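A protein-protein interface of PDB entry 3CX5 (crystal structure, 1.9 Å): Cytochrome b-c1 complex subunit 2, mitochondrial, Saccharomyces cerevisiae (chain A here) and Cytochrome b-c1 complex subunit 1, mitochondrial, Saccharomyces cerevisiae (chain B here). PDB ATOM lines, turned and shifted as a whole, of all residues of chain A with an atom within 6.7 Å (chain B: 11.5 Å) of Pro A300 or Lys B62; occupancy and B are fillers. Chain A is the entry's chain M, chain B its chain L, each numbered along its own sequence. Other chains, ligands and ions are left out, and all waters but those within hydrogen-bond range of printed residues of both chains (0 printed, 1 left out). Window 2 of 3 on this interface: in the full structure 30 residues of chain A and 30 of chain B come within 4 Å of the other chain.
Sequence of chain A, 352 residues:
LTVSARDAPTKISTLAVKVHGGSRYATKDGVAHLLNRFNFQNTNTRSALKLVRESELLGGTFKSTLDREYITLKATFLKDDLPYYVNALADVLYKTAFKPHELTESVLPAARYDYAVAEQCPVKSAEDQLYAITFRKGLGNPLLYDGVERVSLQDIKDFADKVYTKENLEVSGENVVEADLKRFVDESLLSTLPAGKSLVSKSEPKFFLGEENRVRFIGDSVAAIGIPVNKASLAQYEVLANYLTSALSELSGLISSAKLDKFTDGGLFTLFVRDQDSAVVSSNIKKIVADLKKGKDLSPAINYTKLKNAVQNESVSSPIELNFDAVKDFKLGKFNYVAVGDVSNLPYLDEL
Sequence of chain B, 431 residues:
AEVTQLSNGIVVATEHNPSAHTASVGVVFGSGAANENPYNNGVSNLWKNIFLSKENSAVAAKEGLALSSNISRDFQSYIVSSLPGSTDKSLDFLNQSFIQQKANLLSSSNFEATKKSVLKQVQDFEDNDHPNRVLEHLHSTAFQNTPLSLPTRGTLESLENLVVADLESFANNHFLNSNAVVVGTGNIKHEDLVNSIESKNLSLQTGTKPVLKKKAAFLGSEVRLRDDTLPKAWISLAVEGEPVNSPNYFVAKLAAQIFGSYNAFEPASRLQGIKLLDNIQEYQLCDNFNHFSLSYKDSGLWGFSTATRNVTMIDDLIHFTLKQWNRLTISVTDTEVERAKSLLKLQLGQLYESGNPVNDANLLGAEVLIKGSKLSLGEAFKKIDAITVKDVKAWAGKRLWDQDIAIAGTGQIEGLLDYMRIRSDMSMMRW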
ATOM      1  N   TYR A 243      27.074  -8.288 -30.113  1.00  0.00           N
ATOM      2  CA  TYR A 243      28.111  -9.236 -30.512  1.00  0.00           C
ATOM      3  C   TYR A 243      29.485  -8.587 -30.379  1.00  0.00           C
ATOM      4  O   TYR A 243      30.412  -9.176 -29.810  1.00  0.00           O
ATOM      5  CB  TYR A 243      27.886  -9.687 -31.965  1.00  0.00           C
ATOM      6  CG  TYR A 243      29.056 -10.422 -32.591  1.00  0.00           C
ATOM      7  CD1 TYR A 243      29.284 -11.774 -32.329  1.00  0.00           C
ATOM      8  CD2 TYR A 243      29.938  -9.759 -33.445  1.00  0.00           C
ATOM      9  CE1 TYR A 243      30.363 -12.446 -32.903  1.00  0.00           C
ATOM     10  CE2 TYR A 243      31.014 -10.417 -34.022  1.00  0.00           C
ATOM     11  CZ  TYR A 243      31.224 -11.759 -33.747  1.00  0.00           C
ATOM     12  OH  TYR A 243      32.307 -12.397 -34.311  1.00  0.00           O
ATOM     13  N   LEU A 248      31.936 -13.050 -27.331  1.00  0.00           N
ATOM     14  CA  LEU A 248      31.813 -13.814 -28.573  1.00  0.00           C
ATOM     15  C   LEU A 248      32.677 -13.252 -29.695  1.00  0.00           C
ATOM     16  O   LEU A 248      32.953 -13.943 -30.676  1.00  0.00           O
ATOM     17  CB  LEU A 248      30.353 -13.853 -29.033  1.00  0.00           C
ATOM     18  CG  LEU A 248      29.353 -14.473 -28.059  1.00  0.00           C
ATOM     19  CD1 LEU A 248      27.942 -14.223 -28.542  1.00  0.00           C
ATOM     20  CD2 LEU A 248      29.628 -15.958 -27.905  1.00  0.00           C
ATOM     21  N   ASP A 297      29.569 -14.089 -38.908  1.00  0.00           N
ATOM     22  CA  ASP A 297      28.318 -14.736 -38.540  1.00  0.00           C
ATOM     23  C   ASP A 297      27.833 -14.254 -37.168  1.00  0.00           C
ATOM     24  O   ASP A 297      28.476 -14.507 -36.146  1.00  0.00           O
ATOM     25  CB  ASP A 297      28.531 -16.260 -38.545  1.00  0.00           C
ATOM     26  CG  ASP A 297      27.291 -17.039 -38.133  1.00  0.00           C
ATOM     27  OD1 ASP A 297      26.159 -16.619 -38.465  1.00  0.00           O
ATOM     28  OD2 ASP A 297      27.461 -18.092 -37.482  1.00  0.00           O
ATOM     29  N   LEU A 298      26.693 -13.567 -37.164  1.00  0.00           N
ATOM     30  CA  LEU A 298      26.085 -13.024 -35.948  1.00  0.00           C
ATOM     31  C   LEU A 298      25.074 -13.968 -35.298  1.00  0.00           C
ATOM     32  O   LEU A 298      24.472 -13.625 -34.276  1.00  0.00           O
ATOM     33  CB  LEU A 298      25.388 -11.694 -36.257  1.00  0.00           C
ATOM     34  CG  LEU A 298      26.239 -10.591 -36.892  1.00  0.00           C
ATOM     35  CD1 LEU A 298      25.381  -9.364 -37.137  1.00  0.00           C
ATOM     36  CD2 LEU A 298      27.418 -10.256 -35.993  1.00  0.00           C
ATOM     37  N   SER A 299      24.881 -15.145 -35.894  1.00  0.00           N
ATOM     38  CA  SER A 299      23.937 -16.136 -35.368  1.00  0.00           C
ATOM     39  C   SER A 299      24.202 -16.571 -33.925  1.00  0.00           C
ATOM     40  O   SER A 299      23.264 -16.713 -33.144  1.00  0.00           O
ATOM     41  CB  SER A 299      23.886 -17.379 -36.268  1.00  0.00           C
ATOM     42  OG  SER A 299      23.360 -17.072 -37.545  1.00  0.00           O
ATOM     43  N   PRO A 300      25.478 -16.806 -33.556  1.00  0.00           N
ATOM     44  CA  PRO A 300      25.797 -17.227 -32.185  1.00  0.00           C
ATOM     45  C   PRO A 300      25.426 -16.191 -31.122  1.00  0.00           C
ATOM     46  O   PRO A 300      25.284 -16.526 -29.944  1.00  0.00           O
ATOM     47  CB  PRO A 300      27.315 -17.426 -32.235  1.00  0.00           C
ATOM     48  CG  PRO A 300      27.570 -17.783 -33.665  1.00  0.00           C
ATOM     49  CD  PRO A 300      26.696 -16.799 -34.385  1.00  0.00           C
ATOM     50  N   ALA A 301      25.274 -14.938 -31.543  1.00  0.00           N
ATOM     51  CA  ALA A 301      24.938 -13.842 -30.635  1.00  0.00           C
ATOM     52  C   ALA A 301      23.445 -13.540 -30.540  1.00  0.00           C
ATOM     53  O   ALA A 301      23.053 -12.553 -29.919  1.00  0.00           O
ATOM     54  CB  ALA A 301      25.691 -12.587 -31.044  1.00  0.00           C
ATOM     55  N   ILE A 302      22.617 -14.397 -31.134  1.00  0.00           N
ATOM     56  CA  ILE A 302      21.172 -14.196 -31.127  1.00  0.00           C
ATOM     57  C   ILE A 302      20.504 -14.304 -29.752  1.00  0.00           C
ATOM     58  O   ILE A 302      19.786 -13.393 -29.339  1.00  0.00           O
ATOM     59  CB  ILE A 302      20.455 -15.136 -32.148  1.00  0.00           C
ATOM     60  CG1 ILE A 302      18.960 -14.826 -32.192  1.00  0.00           C
ATOM     61  CG2 ILE A 302      20.658 -16.612 -31.779  1.00  0.00           C
ATOM     62  CD1 ILE A 302      18.654 -13.404 -32.587  1.00  0.00           C
ATOM     63  N   ASN A 303      20.728 -15.409 -29.049  1.00  0.00           N
ATOM     64  CA  ASN A 303      20.123 -15.603 -27.731  1.00  0.00           C
ATOM     65  C   ASN A 303      20.618 -14.575 -26.712  1.00  0.00           C
ATOM     66  O   ASN A 303      19.869 -14.145 -25.832  1.00  0.00           O
ATOM     67  CB  ASN A 303      20.387 -17.026 -27.226  1.00  0.00           C
ATOM     68  CG  ASN A 303      19.659 -18.082 -28.046  1.00  0.00           C
ATOM     69  OD1 ASN A 303      18.632 -17.807 -28.668  1.00  0.00           O
ATOM     70  ND2 ASN A 303      20.190 -19.300 -28.047  1.00  0.00           N
ATOM     71  N   TYR A 304      21.876 -14.171 -26.863  1.00  0.00           N
ATOM     72  CA  TYR A 304      22.503 -13.193 -25.981  1.00  0.00           C
ATOM     73  C   TYR A 304      21.860 -11.822 -26.174  1.00  0.00           C
ATOM     74  O   TYR A 304      21.495 -11.165 -25.198  1.00  0.00           O
ATOM     75  CB  TYR A 304      24.004 -13.130 -26.268  1.00  0.00           C
ATOM     76  CG  TYR A 304      24.785 -12.160 -25.408  1.00  0.00           C
ATOM     77  CD1 TYR A 304      25.416 -11.057 -25.979  1.00  0.00           C
ATOM     78  CD2 TYR A 304      24.938 -12.370 -24.036  1.00  0.00           C
ATOM     79  CE1 TYR A 304      26.186 -10.186 -25.213  1.00  0.00           C
ATOM     80  CE2 TYR A 304      25.708 -11.504 -23.258  1.00  0.00           C
ATOM     81  CZ  TYR A 304      26.331 -10.414 -23.858  1.00  0.00           C
ATOM     82  OH  TYR A 304      27.107  -9.550 -23.117  1.00  0.00           O
ATOM     83  N   LYS A 328      21.751 -13.307 -39.488  1.00  0.00           N
ATOM     84  CA  LYS A 328      22.813 -14.296 -39.577  1.00  0.00           C
ATOM     85  C   LYS A 328      24.158 -13.678 -39.927  1.00  0.00           C
ATOM     86  O   LYS A 328      25.073 -13.681 -39.112  1.00  0.00           O
ATOM     87  CB  LYS A 328      22.469 -15.401 -40.586  1.00  0.00           C
ATOM     88  CG  LYS A 328      23.511 -16.521 -40.625  1.00  0.00           C
ATOM     89  CD  LYS A 328      23.112 -17.672 -41.535  1.00  0.00           C
ATOM     90  CE  LYS A 328      24.172 -18.773 -41.512  1.00  0.00           C
ATOM     91  NZ  LYS A 328      23.814 -19.937 -42.375  1.00  0.00           N
ATOM     92  N   SER B  53      35.752 -13.658 -16.776  1.00  0.00           N
ATOM     93  CA  SER B  53      36.788 -13.857 -17.785  1.00  0.00           C
ATOM     94  C   SER B  53      36.171 -14.120 -19.162  1.00  0.00           C
ATOM     95  O   SER B  53      35.072 -14.667 -19.266  1.00  0.00           O
ATOM     96  CB  SER B  53      37.681 -15.025 -17.372  1.00  0.00           C
ATOM     97  OG  SER B  53      38.833 -15.095 -18.186  1.00  0.00           O
ATOM     98  N   LYS B  54      36.894 -13.741 -20.213  1.00  0.00           N
ATOM     99  CA  LYS B  54      36.412 -13.904 -21.581  1.00  0.00           C
ATOM    100  C   LYS B  54      36.013 -15.336 -21.942  1.00  0.00           C
ATOM    101  O   LYS B  54      34.966 -15.551 -22.554  1.00  0.00           O
ATOM    102  CB  LYS B  54      37.438 -13.369 -22.580  1.00  0.00           C
ATOM    103  CG  LYS B  54      36.866 -13.159 -23.974  1.00  0.00           C
ATOM    104  CD  LYS B  54      37.869 -12.508 -24.914  1.00  0.00           C
ATOM    105  CE  LYS B  54      37.236 -12.237 -26.274  1.00  0.00           C
ATOM    106  NZ  LYS B  54      38.188 -11.578 -27.215  1.00  0.00           N
ATOM    107  N   GLU B  55      36.843 -16.304 -21.554  1.00  0.00           N
ATOM    108  CA  GLU B  55      36.578 -17.717 -21.830  1.00  0.00           C
ATOM    109  C   GLU B  55      35.238 -18.120 -21.223  1.00  0.00           C
ATOM    110  O   GLU B  55      34.385 -18.697 -21.896  1.00  0.00           O
ATOM    111  CB  GLU B  55      37.674 -18.603 -21.222  1.00  0.00           C
ATOM    112  CG  GLU B  55      39.094 -18.327 -21.711  1.00  0.00           C
ATOM    113  CD  GLU B  55      40.144 -19.198 -21.018  1.00  0.00           C
ATOM    114  OE1 GLU B  55      39.839 -19.797 -19.961  1.00  0.00           O
ATOM    115  OE2 GLU B  55      41.283 -19.277 -21.531  1.00  0.00           O
ATOM    116  N   ASN B  56      35.066 -17.796 -19.944  1.00  0.00           N
ATOM    117  CA  ASN B  56      33.849 -18.119 -19.210  1.00  0.00           C
ATOM    118  C   ASN B  56      32.638 -17.343 -19.731  1.00  0.00           C
ATOM    119  O   ASN B  56      31.542 -17.896 -19.834  1.00  0.00           O
ATOM    120  CB  ASN B  56      34.056 -17.839 -17.719  1.00  0.00           C
ATOM    121  CG  ASN B  56      33.292 -18.808 -16.832  1.00  0.00           C
ATOM    122  OD1 ASN B  56      33.265 -20.012 -17.086  1.00  0.00           O
ATOM    123  ND2 ASN B  56      32.682 -18.287 -15.774  1.00  0.00           N
ATOM    124  N   SER B  57      32.843 -16.071 -20.067  1.00  0.00           N
ATOM    125  CA  SER B  57      31.771 -15.220 -20.581  1.00  0.00           C
ATOM    126  C   SER B  57      31.270 -15.678 -21.951  1.00  0.00           C
ATOM    127  O   SER B  57      30.088 -15.524 -22.266  1.00  0.00           O
ATOM    128  CB  SER B  57      32.225 -13.757 -20.658  1.00  0.00           C
ATOM    129  OG  SER B  57      32.430 -13.208 -19.367  1.00  0.00           O
ATOM    130  N   ALA B  58      32.177 -16.218 -22.764  1.00  0.00           N
ATOM    131  CA  ALA B  58      31.826 -16.707 -24.098  1.00  0.00           C
ATOM    132  C   ALA B  58      30.890 -17.912 -23.997  1.00  0.00           C
ATOM    133  O   ALA B  58      29.900 -17.999 -24.725  1.00  0.00           O
ATOM    134  CB  ALA B  58      33.081 -17.067 -24.878  1.00  0.00           C
ATOM    135  N   VAL B  59      31.189 -18.826 -23.075  1.00  0.00           N
ATOM    136  CA  VAL B  59      30.353 -20.008 -22.873  1.00  0.00           C
ATOM    137  C   VAL B  59      28.958 -19.559 -22.456  1.00  0.00           C
ATOM    138  O   VAL B  59      27.956 -20.038 -22.988  1.00  0.00           O
ATOM    139  CB  VAL B  59      30.935 -20.935 -21.780  1.00  0.00           C
ATOM    140  CG1 VAL B  59      29.978 -22.085 -21.490  1.00  0.00           C
ATOM    141  CG2 VAL B  59      32.286 -21.473 -22.219  1.00  0.00           C
ATOM    142  N   ALA B  60      28.907 -18.609 -21.527  1.00  0.00           N
ATOM    143  CA  ALA B  60      27.642 -18.076 -21.030  1.00  0.00           C
ATOM    144  C   ALA B  60      26.860 -17.352 -22.128  1.00  0.00           C
ATOM    145  O   ALA B  60      25.648 -17.532 -22.253  1.00  0.00           O
ATOM    146  CB  ALA B  60      27.898 -17.137 -19.848  1.00  0.00           C
ATOM    147  N   ALA B  61      27.562 -16.556 -22.932  1.00  0.00           N
ATOM    148  CA  ALA B  61      26.938 -15.801 -24.019  1.00  0.00           C
ATOM    149  C   ALA B  61      26.329 -16.709 -25.093  1.00  0.00           C
ATOM    150  O   ALA B  61      25.290 -16.385 -25.673  1.00  0.00           O
ATOM    151  CB  ALA B  61      27.949 -14.858 -24.648  1.00  0.00           C
ATOM    152  N   LYS B  62      26.993 -17.833 -25.363  1.00  0.00           N
ATOM    153  CA  LYS B  62      26.520 -18.800 -26.355  1.00  0.00           C
ATOM    154  C   LYS B  62      25.137 -19.322 -25.963  1.00  0.00           C
ATOM    155  O   LYS B  62      24.290 -19.580 -26.819  1.00  0.00           O
ATOM    156  CB  LYS B  62      27.503 -19.972 -26.462  1.00  0.00           C
ATOM    157  CG  LYS B  62      28.750 -19.703 -27.295  1.00  0.00           C
ATOM    158  CD  LYS B  62      28.459 -19.893 -28.774  1.00  0.00           C
ATOM    159  CE  LYS B  62      29.729 -19.858 -29.609  1.00  0.00           C
ATOM    160  NZ  LYS B  62      29.444 -20.200 -31.035  1.00  0.00           N
ATOM    161  N   GLU B  63      24.922 -19.460 -24.658  1.00  0.00           N
ATOM    162  CA  GLU B  63      23.661 -19.942 -24.110  1.00  0.00           C
ATOM    163  C   GLU B  63      22.674 -18.809 -23.808  1.00  0.00           C
ATOM    164  O   GLU B  63      21.615 -19.042 -23.214  1.00  0.00           O
ATOM    165  CB  GLU B  63      23.928 -20.749 -22.833  1.00  0.00           C
ATOM    166  CG  GLU B  63      24.046 -22.261 -23.031  1.00  0.00           C
ATOM    167  CD  GLU B  63      25.129 -22.671 -24.015  1.00  0.00           C
ATOM    168  OE1 GLU B  63      26.312 -22.324 -23.792  1.00  0.00           O
ATOM    169  OE2 GLU B  63      24.796 -23.357 -25.008  1.00  0.00           O
ATOM    170  N   GLY B  64      23.019 -17.590 -24.224  1.00  0.00           N
ATOM    171  CA  GLY B  64      22.163 -16.439 -23.974  1.00  0.00           C
ATOM    172  C   GLY B  64      22.145 -16.027 -22.507  1.00  0.00           C
ATOM    173  O   GLY B  64      21.100 -15.656 -21.963  1.00  0.00           O
ATOM    174  N   LEU B  65      23.309 -16.104 -21.868  1.00  0.00           N
ATOM    175  CA  LEU B  65      23.459 -15.760 -20.457  1.00  0.00           C
ATOM    176  C   LEU B  65      24.421 -14.585 -20.239  1.00  0.00           C
ATOM    177  O   LEU B  65      25.407 -14.427 -20.969  1.00  0.00           O
ATOM    178  CB  LEU B  65      23.960 -16.985 -19.681  1.00  0.00           C
ATOM    179  CG  LEU B  65      22.997 -18.071 -19.175  1.00  0.00           C
ATOM    180  CD1 LEU B  65      21.847 -18.321 -20.119  1.00  0.00           C
ATOM    181  CD2 LEU B  65      23.781 -19.351 -18.927  1.00  0.00           C
ATOM    182  N   ALA B  66      24.122 -13.763 -19.235  1.00  0.00           N
ATOM    183  CA  ALA B  66      24.957 -12.611 -18.892  1.00  0.00           C
ATOM    184  C   ALA B  66      25.493 -12.798 -17.477  1.00  0.00           C
ATOM    185  O   ALA B  66      24.745 -13.144 -16.561  1.00  0.00           O
ATOM    186  CB  ALA B  66      24.158 -11.325 -18.990  1.00  0.00           C
ATOM    187  N   LEU B  67      26.790 -12.568 -17.303  1.00  0.00           N
ATOM    188  CA  LEU B  67      27.429 -12.738 -15.998  1.00  0.00           C
ATOM    189  C   LEU B  67      27.625 -11.456 -15.191  1.00  0.00           C
ATOM    190  O   LEU B  67      27.955 -10.404 -15.741  1.00  0.00           O
ATOM    191  CB  LEU B  67      28.775 -13.444 -16.165  1.00  0.00           C
ATOM    192  CG  LEU B  67      28.741 -14.773 -16.922  1.00  0.00           C
ATOM    193  CD1 LEU B  67      30.146 -15.344 -17.014  1.00  0.00           C
ATOM    194  CD2 LEU B  67      27.802 -15.744 -16.219  1.00  0.00           C
ATOM    195  N   VAL B  80      24.064 -15.092 -12.684  1.00  0.00           N
ATOM    196  CA  VAL B  80      23.862 -15.381 -14.096  1.00  0.00           C
ATOM    197  C   VAL B  80      22.449 -14.951 -14.466  1.00  0.00           C
ATOM    198  O   VAL B  80      21.475 -15.361 -13.825  1.00  0.00           O
ATOM    199  CB  VAL B  80      24.020 -16.893 -14.409  1.00  0.00           C
ATOM    200  CG1 VAL B  80      24.020 -17.111 -15.914  1.00  0.00           C
ATOM    201  CG2 VAL B  80      25.306 -17.442 -13.793  1.00  0.00           C
ATOM    202  N   SER B  81      22.345 -14.094 -15.475  1.00  0.00           N
ATOM    203  CA  SER B  81      21.050 -13.611 -15.930  1.00  0.00           C
ATOM    204  C   SER B  81      20.656 -14.260 -17.253  1.00  0.00           C
ATOM    205  O   SER B  81      21.513 -14.575 -18.091  1.00  0.00           O
ATOM    206  CB  SER B  81      21.066 -12.087 -16.069  1.00  0.00           C
ATOM    207  OG  SER B  81      21.268 -11.471 -14.809  1.00  0.00           O
ATOM    208  N   SER B  82      19.350 -14.444 -17.433  1.00  0.00           N
ATOM    209  CA  SER B  82      18.800 -15.058 -18.637  1.00  0.00           C
ATOM    210  C   SER B  82      17.312 -14.750 -18.732  1.00  0.00           C
ATOM    211  O   SER B  82      16.732 -14.173 -17.814  1.00  0.00           O
ATOM    212  CB  SER B  82      18.965 -16.580 -18.566  1.00  0.00           C
ATOM    213  OG  SER B  82      18.115 -17.138 -17.566  1.00  0.00           O
ATOM    214  N   LEU B  83      16.698 -15.147 -19.843  1.00  0.00           N
ATOM    215  CA  LEU B  83      15.263 -14.963 -20.029  1.00  0.00           C
ATOM    216  C   LEU B  83      14.602 -15.909 -19.028  1.00  0.00           C
ATOM    217  O   LEU B  83      15.215 -16.894 -18.608  1.00  0.00           O
ATOM    218  CB  LEU B  83      14.855 -15.329 -21.457  1.00  0.00           C
ATOM    219  CG  LEU B  83      15.388 -14.400 -22.548  1.00  0.00           C
ATOM    220  CD1 LEU B  83      14.997 -14.937 -23.917  1.00  0.00           C
ATOM    221  CD2 LEU B  83      14.845 -12.985 -22.345  1.00  0.00           C
ATOM    222  N   SER B  86      14.913 -19.682 -19.569  1.00  0.00           N
ATOM    223  CA  SER B  86      16.237 -20.302 -19.585  1.00  0.00           C
ATOM    224  C   SER B  86      16.900 -20.381 -18.209  1.00  0.00           C
ATOM    225  O   SER B  86      18.128 -20.434 -18.106  1.00  0.00           O
ATOM    226  CB  SER B  86      17.152 -19.557 -20.560  1.00  0.00           C
ATOM    227  OG  SER B  86      16.605 -19.539 -21.867  1.00  0.00           O
ATOM    228  N   LYS B  89      19.282 -23.295 -17.809  1.00  0.00           N
ATOM    229  CA  LYS B  89      20.591 -23.134 -18.429  1.00  0.00           C
ATOM    230  C   LYS B  89      21.543 -22.332 -17.532  1.00  0.00           C
ATOM    231  O   LYS B  89      22.765 -22.497 -17.606  1.00  0.00           O
ATOM    232  CB  LYS B  89      20.438 -22.466 -19.799  1.00  0.00           C
ATOM    233  CG  LYS B  89      21.330 -23.063 -20.872  1.00  0.00           C
ATOM    234  CD  LYS B  89      21.090 -24.567 -21.018  1.00  0.00           C
ATOM    235  CE  LYS B  89      22.102 -25.223 -21.957  1.00  0.00           C
ATOM    236  NZ  LYS B  89      21.998 -24.721 -23.361  1.00  0.00           N
ATOM    237  N   SER B  90      20.974 -21.485 -16.675  1.00  0.00           N
ATOM    238  CA  SER B  90      21.753 -20.671 -15.744  1.00  0.00           C
ATOM    239  C   SER B  90      22.349 -21.559 -14.658  1.00  0.00           C
ATOM    240  O   SER B  90      23.525 -21.430 -14.316  1.00  0.00           O
ATOM    241  CB  SER B  90      20.874 -19.596 -15.101  1.00  0.00           C
ATOM    242  OG  SER B  90      20.376 -18.697 -16.073  1.00  0.00           O
ATOM    243  N   PHE B  93      25.209 -23.697 -15.808  1.00  0.00           N
ATOM    244  CA  PHE B  93      26.438 -22.920 -15.919  1.00  0.00           C
ATOM    245  C   PHE B  93      27.029 -22.722 -14.528  1.00  0.00           C
ATOM    246  O   PHE B  93      28.236 -22.846 -14.329  1.00  0.00           O
ATOM    247  CB  PHE B  93      26.155 -21.559 -16.558  1.00  0.00           C
ATOM    248  CG  PHE B  93      27.387 -20.729 -16.775  1.00  0.00           C
ATOM    249  CD1 PHE B  93      28.082 -20.798 -17.979  1.00  0.00           C
ATOM    250  CD2 PHE B  93      27.867 -19.892 -15.767  1.00  0.00           C
ATOM    251  CE1 PHE B  93      29.240 -20.050 -18.179  1.00  0.00           C
ATOM    252  CE2 PHE B  93      29.024 -19.142 -15.955  1.00  0.00           C
ATOM    253  CZ  PHE B  93      29.713 -19.220 -17.163  1.00  0.00           C
ATOM    254  N   GLN B  96      28.713 -25.812 -13.299  1.00  0.00           N
ATOM    255  CA  GLN B  96      30.010 -26.013 -13.938  1.00  0.00           C
ATOM    256  C   GLN B  96      31.083 -25.080 -13.374  1.00  0.00           C
ATOM    257  O   GLN B  96      32.261 -25.442 -13.324  1.00  0.00           O
ATOM    258  CB  GLN B  96      29.892 -25.798 -15.451  1.00  0.00           C
ATOM    259  CG  GLN B  96      31.220 -25.902 -16.198  1.00  0.00           C
ATOM    260  CD  GLN B  96      31.108 -25.546 -17.670  1.00  0.00           C
ATOM    261  OE1 GLN B  96      30.695 -24.439 -18.027  1.00  0.00           O
ATOM    262  NE2 GLN B  96      31.493 -26.480 -18.536  1.00  0.00           N
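N of Leu B65 lies within hydrogen-bond range of O of Ala B60, 2.8 Å away.
CD2 of Leu A248 touches O of Ala B58 (3.8 Å). CB of Ala B61 touches CG of Leu A248, at 3.7 Å. Leu A248 touches Lys B62 (CD2 to CG, 3.9 Å). Pro A300 touches Lys B62 (CB to NZ, 3.7 Å). C of Asn A303 touches CA of Gly B64, at 3.7 Å. Ala B61 touches Tyr A304. N of Tyr A304 touches CA of Gly B64, at 3.7 Å. Tyr A304 touches Leu B65 (CD2 to O, 3.7 Å).
Leu A248 touches just these residues of chain B: Ala B58, Ala B61 and Lys B62. No residue of chain B comes within 4 Å of Asp A297. Ser A299 touches none of the printed residues of chain B. Of the printed residues of chain B, Pro A300 touches Lys B62. No residue of chain B comes within 4 Å of Ala A301. Asn A303 touches just one residue of chain B: Gly B64 (3.7 Å). Of the printed residues of chain A, Ala B58 touches Leu A248 (3.8 Å). Of chain A, only Leu A248 (3.9 Å) and Pro A300 (3.7 Å) come within 4 Å of Lys B62. Printed residues of chain A within 4 Å of Gly B64: Asn A303 (3.7 Å) and Tyr A304 (3.7 Å). The nearest residue of chain B that does not touch Pro A300 is Ala B61 (4.3 Å). The nearest residue of chain A that does not touch Lys B62 is Asn A303 (4.3 Å). The nearest printed residue of chain A that does not touch Ala B58 is Pro A300 (7.1 Å).
Of the 11 printed residues of chain A, 4 touch a printed residue of chain B. Hydrophobic or aromatic side chains of chain A that line the printed part of chain B: Leu A248, Pro A300 and Tyr A304. Of the 24 printed residues of chain B, 5 touch a printed residue of chain A. Hydrophobic or aromatic side chains of chain B that line the printed part of chain A: Ala B61. Along chain B the printed residues that touch a printed residue of chain A span positions 58 to 65. Among the printed residues, 8 pairs touch across the chains.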
